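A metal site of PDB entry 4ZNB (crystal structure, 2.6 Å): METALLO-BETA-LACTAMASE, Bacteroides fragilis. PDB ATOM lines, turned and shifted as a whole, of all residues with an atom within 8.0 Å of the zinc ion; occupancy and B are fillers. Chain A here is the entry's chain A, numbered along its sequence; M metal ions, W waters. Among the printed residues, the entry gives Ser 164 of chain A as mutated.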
ATOM      1  N   ASP A  52      13.143  -4.380  13.265  1.00  0.00           N
ATOM      2  CA  ASP A  52      14.290  -4.722  14.138  1.00  0.00           C
ATOM      3  C   ASP A  52      14.660  -6.193  13.902  1.00  0.00           C
ATOM      4  O   ASP A  52      13.811  -7.009  13.568  1.00  0.00           O
ATOM      5  CB  ASP A  52      13.949  -4.615  15.655  1.00  0.00           C
ATOM      6  CG  ASP A  52      14.105  -3.196  16.238  1.00  0.00           C
ATOM      7  OD1 ASP A  52      14.049  -2.196  15.506  1.00  0.00           O
ATOM      8  OD2 ASP A  52      14.247  -3.107  17.467  1.00  0.00           O
ATOM      9  N   ASN A  81      15.118   0.384  14.596  1.00  0.00           N
ATOM     10  CA  ASN A  81      14.773   1.455  15.517  1.00  0.00           C
ATOM     11  C   ASN A  81      15.903   2.457  15.530  1.00  0.00           C
ATOM     12  O   ASN A  81      15.671   3.655  15.415  1.00  0.00           O
ATOM     13  CB  ASN A  81      14.514   0.918  16.923  1.00  0.00           C
ATOM     14  CG  ASN A  81      13.831   1.941  17.813  1.00  0.00           C
ATOM     15  OD1 ASN A  81      14.488   2.647  18.597  1.00  0.00           O
ATOM     16  ND2 ASN A  81      12.504   2.067  17.661  1.00  0.00           N
ATOM     17  N   HIS A  82      17.109   1.945  15.707  1.00  0.00           N
ATOM     18  CA  HIS A  82      18.326   2.736  15.725  1.00  0.00           C
ATOM     19  C   HIS A  82      19.468   1.817  15.315  1.00  0.00           C
ATOM     20  O   HIS A  82      19.212   0.707  14.854  1.00  0.00           O
ATOM     21  CB  HIS A  82      18.587   3.391  17.091  1.00  0.00           C
ATOM     22  CG  HIS A  82      18.430   2.456  18.257  1.00  0.00           C
ATOM     23  ND1 HIS A  82      17.222   1.932  18.664  1.00  0.00           N
ATOM     24  CD2 HIS A  82      19.346   1.975  19.125  1.00  0.00           C
ATOM     25  CE1 HIS A  82      17.439   1.183  19.746  1.00  0.00           C
ATOM     26  NE2 HIS A  82      18.711   1.169  20.077  1.00  0.00           N
ATOM     27  N   TRP A  83      20.704   2.232  15.541  1.00  0.00           N
ATOM     28  CA  TRP A  83      21.850   1.433  15.111  1.00  0.00           C
ATOM     29  C   TRP A  83      22.335   0.300  15.980  1.00  0.00           C
ATOM     30  O   TRP A  83      23.203  -0.465  15.564  1.00  0.00           O
ATOM     31  CB  TRP A  83      23.033   2.351  14.814  1.00  0.00           C
ATOM     32  CG  TRP A  83      23.532   3.056  16.019  1.00  0.00           C
ATOM     33  CD1 TRP A  83      23.102   4.255  16.519  1.00  0.00           C
ATOM     34  CD2 TRP A  83      24.620   2.640  16.850  1.00  0.00           C
ATOM     35  NE1 TRP A  83      23.880   4.622  17.599  1.00  0.00           N
ATOM     36  CE2 TRP A  83      24.812   3.651  17.824  1.00  0.00           C
ATOM     37  CE3 TRP A  83      25.470   1.512  16.863  1.00  0.00           C
ATOM     38  CZ2 TRP A  83      25.813   3.567  18.797  1.00  0.00           C
ATOM     39  CZ3 TRP A  83      26.460   1.424  17.823  1.00  0.00           C
ATOM     40  CH2 TRP A  83      26.621   2.445  18.782  1.00  0.00           C
ATOM     41  N   HIS A  84      21.821   0.211  17.196  1.00  0.00           N
ATOM     42  CA  HIS A  84      22.249  -0.873  18.070  1.00  0.00           C
ATOM     43  C   HIS A  84      21.959  -2.283  17.547  1.00  0.00           C
ATOM     44  O   HIS A  84      21.031  -2.476  16.771  1.00  0.00           O
ATOM     45  CB  HIS A  84      21.724  -0.647  19.492  1.00  0.00           C
ATOM     46  CG  HIS A  84      22.427   0.475  20.181  1.00  0.00           C
ATOM     47  ND1 HIS A  84      21.871   1.181  21.222  1.00  0.00           N
ATOM     48  CD2 HIS A  84      23.635   1.053  19.943  1.00  0.00           C
ATOM     49  CE1 HIS A  84      22.702   2.139  21.591  1.00  0.00           C
ATOM     50  NE2 HIS A  84      23.789   2.073  20.835  1.00  0.00           N
ATOM     51  N   GLY A  85      22.817  -3.227  17.923  1.00  0.00           N
ATOM     52  CA  GLY A  85      22.698  -4.617  17.485  1.00  0.00           C
ATOM     53  C   GLY A  85      21.344  -5.297  17.641  1.00  0.00           C
ATOM     54  O   GLY A  85      20.998  -6.177  16.851  1.00  0.00           O
ATOM     55  N   ASP A  86      20.607  -4.939  18.686  1.00  0.00           N
ATOM     56  CA  ASP A  86      19.288  -5.502  18.918  1.00  0.00           C
ATOM     57  C   ASP A  86      18.318  -4.933  17.873  1.00  0.00           C
ATOM     58  O   ASP A  86      17.114  -5.158  17.945  1.00  0.00           O
ATOM     59  CB  ASP A  86      18.799  -5.223  20.361  1.00  0.00           C
ATOM     60  CG  ASP A  86      18.809  -3.724  20.759  1.00  0.00           C
ATOM     61  OD1 ASP A  86      19.799  -3.023  20.474  1.00  0.00           O
ATOM     62  OD2 ASP A  86      17.847  -3.244  21.402  1.00  0.00           O
ATOM     63  N   CYS A  87      18.852  -4.217  16.875  1.00  0.00           N
ATOM     64  CA  CYS A  87      18.062  -3.632  15.802  1.00  0.00           C
ATOM     65  C   CYS A  87      18.549  -4.079  14.434  1.00  0.00           C
ATOM     66  O   CYS A  87      17.762  -4.532  13.614  1.00  0.00           O
ATOM     67  CB  CYS A  87      18.119  -2.115  15.862  1.00  0.00           C
ATOM     68  SG  CYS A  87      17.443  -1.379  17.369  1.00  0.00           S
ATOM     69  N   HIS A 145      16.753   6.932  23.604  1.00  0.00           N
ATOM     70  CA  HIS A 145      17.633   5.855  24.071  1.00  0.00           C
ATOM     71  C   HIS A 145      18.918   5.970  23.287  1.00  0.00           C
ATOM     72  O   HIS A 145      20.009   5.662  23.791  1.00  0.00           O
ATOM     73  CB  HIS A 145      16.978   4.509  23.783  1.00  0.00           C
ATOM     74  CG  HIS A 145      17.938   3.370  23.793  1.00  0.00           C
ATOM     75  ND1 HIS A 145      18.364   2.759  24.958  1.00  0.00           N
ATOM     76  CD2 HIS A 145      18.592   2.762  22.780  1.00  0.00           C
ATOM     77  CE1 HIS A 145      19.254   1.826  24.661  1.00  0.00           C
ATOM     78  NE2 HIS A 145      19.419   1.811  23.344  1.00  0.00           N
ATOM     79  N   ALA A 146      18.761   6.352  22.027  1.00  0.00           N
ATOM     80  CA  ALA A 146      19.845   6.559  21.090  1.00  0.00           C
ATOM     81  C   ALA A 146      19.521   7.876  20.407  1.00  0.00           C
ATOM     82  O   ALA A 146      18.367   8.280  20.307  1.00  0.00           O
ATOM     83  CB  ALA A 146      19.893   5.439  20.058  1.00  0.00           C
ATOM     84  N   ASP A 148      19.598   8.552  17.339  1.00  0.00           N
ATOM     85  CA  ASP A 148      18.803   8.291  16.133  1.00  0.00           C
ATOM     86  C   ASP A 148      17.479   7.553  16.215  1.00  0.00           C
ATOM     87  O   ASP A 148      16.812   7.424  15.195  1.00  0.00           O
ATOM     88  CB  ASP A 148      19.674   7.550  15.141  1.00  0.00           C
ATOM     89  CG  ASP A 148      20.079   6.201  15.659  1.00  0.00           C
ATOM     90  OD1 ASP A 148      20.237   6.074  16.873  1.00  0.00           O
ATOM     91  OD2 ASP A 148      20.223   5.257  14.868  1.00  0.00           O
ATOM     92  N   ASN A 149      17.063   7.144  17.406  1.00  0.00           N
ATOM     93  CA  ASN A 149      15.831   6.363  17.538  1.00  0.00           C
ATOM     94  C   ASN A 149      14.524   6.927  16.938  1.00  0.00           C
ATOM     95  O   ASN A 149      14.230   8.129  16.996  1.00  0.00           O
ATOM     96  CB  ASN A 149      15.635   5.823  18.983  1.00  0.00           C
ATOM     97  CG  ASN A 149      15.712   6.902  20.075  1.00  0.00           C
ATOM     98  OD1 ASN A 149      16.104   6.624  21.201  1.00  0.00           O
ATOM     99  ND2 ASN A 149      15.299   8.104  19.755  1.00  0.00           N
ATOM    100  N   GLY A 163      10.114   0.839  20.308  1.00  0.00           N
ATOM    101  CA  GLY A 163      11.522   0.540  20.360  1.00  0.00           C
ATOM    102  C   GLY A 163      12.099   0.703  21.758  1.00  0.00           C
ATOM    103  O   GLY A 163      11.357   0.956  22.721  1.00  0.00           O
ATOM    104  N   SER A 164      13.422   0.590  21.861  1.00  0.00           N
ATOM    105  CA  SER A 164      14.124   0.697  23.135  1.00  0.00           C
ATOM    106  C   SER A 164      14.042   2.060  23.797  1.00  0.00           C
ATOM    107  O   SER A 164      14.626   2.245  24.861  1.00  0.00           O
ATOM    108  CB  SER A 164      15.602   0.298  22.957  1.00  0.00           C
ATOM    109  OG  SER A 164      15.728  -0.916  22.251  1.00  0.00           O
ATOM    110  N   MET A 165      13.394   3.048  23.182  1.00  0.00           N
ATOM    111  CA  MET A 165      13.281   4.333  23.876  1.00  0.00           C
ATOM    112  C   MET A 165      12.203   4.148  24.955  1.00  0.00           C
ATOM    113  O   MET A 165      12.053   4.992  25.843  1.00  0.00           O
ATOM    114  CB  MET A 165      12.901   5.485  22.941  1.00  0.00           C
ATOM    115  CG  MET A 165      11.435   5.609  22.610  1.00  0.00           C
ATOM    116  SD  MET A 165      11.032   7.258  21.946  1.00  0.00           S
ATOM    117  CE  MET A 165      11.600   7.070  20.240  1.00  0.00           C
ATOM    118  N   ASN A 176      21.260   1.292  29.392  1.00  0.00           N
ATOM    119  CA  ASN A 176      22.393   1.820  28.637  1.00  0.00           C
ATOM    120  C   ASN A 176      22.130   3.203  28.014  1.00  0.00           C
ATOM    121  O   ASN A 176      21.311   3.368  27.110  1.00  0.00           O
ATOM    122  CB  ASN A 176      22.816   0.807  27.572  1.00  0.00           C
ATOM    123  CG  ASN A 176      23.881   1.361  26.634  1.00  0.00           C
ATOM    124  OD1 ASN A 176      24.821   2.005  27.080  1.00  0.00           O
ATOM    125  ND2 ASN A 176      23.741   1.091  25.342  1.00  0.00           N
ATOM    126  N   ASP A 179      24.622   5.909  24.141  1.00  0.00           N
ATOM    127  CA  ASP A 179      24.357   6.707  22.963  1.00  0.00           C
ATOM    128  C   ASP A 179      22.991   7.371  23.092  1.00  0.00           C
ATOM    129  O   ASP A 179      22.322   7.673  22.098  1.00  0.00           O
ATOM    130  CB  ASP A 179      24.447   5.815  21.714  1.00  0.00           C
ATOM    131  CG  ASP A 179      25.733   4.984  21.679  1.00  0.00           C
ATOM    132  OD1 ASP A 179      25.753   3.855  22.242  1.00  0.00           O
ATOM    133  OD2 ASP A 179      26.738   5.456  21.096  1.00  0.00           O
ATOM    134  N   GLY A 205      11.477  -1.826  23.458  1.00  0.00           N
ATOM    135  CA  GLY A 205      12.663  -2.460  22.925  1.00  0.00           C
ATOM    136  C   GLY A 205      12.996  -3.774  23.598  1.00  0.00           C
ATOM    137  O   GLY A 205      13.469  -4.706  22.966  1.00  0.00           O
ATOM    138  N   HIS A 206      12.784  -3.837  24.903  1.00  0.00           N
ATOM    139  CA  HIS A 206      13.065  -5.028  25.683  1.00  0.00           C
ATOM    140  C   HIS A 206      11.956  -5.159  26.724  1.00  0.00           C
ATOM    141  O   HIS A 206      11.633  -4.198  27.424  1.00  0.00           O
ATOM    142  CB  HIS A 206      14.425  -4.906  26.393  1.00  0.00           C
ATOM    143  CG  HIS A 206      15.556  -4.490  25.496  1.00  0.00           C
ATOM    144  ND1 HIS A 206      16.394  -5.402  24.880  1.00  0.00           N
ATOM    145  CD2 HIS A 206      15.994  -3.266  25.122  1.00  0.00           C
ATOM    146  CE1 HIS A 206      17.297  -4.748  24.169  1.00  0.00           C
ATOM    147  NE2 HIS A 206      17.076  -3.454  24.298  1.00  0.00           N
HETATM  148 ZN    ZN M   1      19.793   0.343  21.768  1.00  0.00          ZN
HETATM  149  O   HOH W   1      19.582  -1.779  23.019  1.00  0.00           O
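The side-chain amide oxygen (OD1) of Asn 149 sits at hydrogen-bond distance from the backbone NH (N) of His 145, 2.5 Å away. The side-chain carboxylate (OD2) of Asp 86 sits at hydrogen-bond distance from a ring nitrogen (NE2) of His 206 (3.0 Å). OD1 of Asn 81 is in hydrogen-bond range of ND1 of His 82 (2.8 Å). A ring nitrogen (ND1) of His 82 sits close to the side-chain sulfur (SG) of Cys 87 (3.6 Å). OD1 of Asp 179 sits at hydrogen-bond distance from NE2 of His 84 (3.0 Å). The backbone carbonyl oxygen of His 84 lies close to the side-chain sulfur of Cys 87 (3.8 Å). The side-chain carboxylate of Asp 86 lies within hydrogen-bond range of the side-chain hydroxyl of Ser 164 (3.3 Å).
Merely in contact with the zinc ion: Asp 86 (3.6 Å). Four residues have an atom within 4 Å of the zinc ion: His 82, His 84, Asp 86 and His 145. The nearest printed residue that does not touch the zinc ion is Ser 164 (4.3 Å).
The zinc ion is bound by a ring nitrogen (NE2) of His 82 (2.2 Å), a ring nitrogen (NE2) of His 145 (2.2 Å), a ring nitrogen (ND1) of His 84 (2.3 Å) and water W1 (2.5 Å).
Water W1 bridges the side-chain carboxylate of Asp 86 (2.8 Å) and a ring nitrogen (NE2) of His 206 (3.3 Å).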
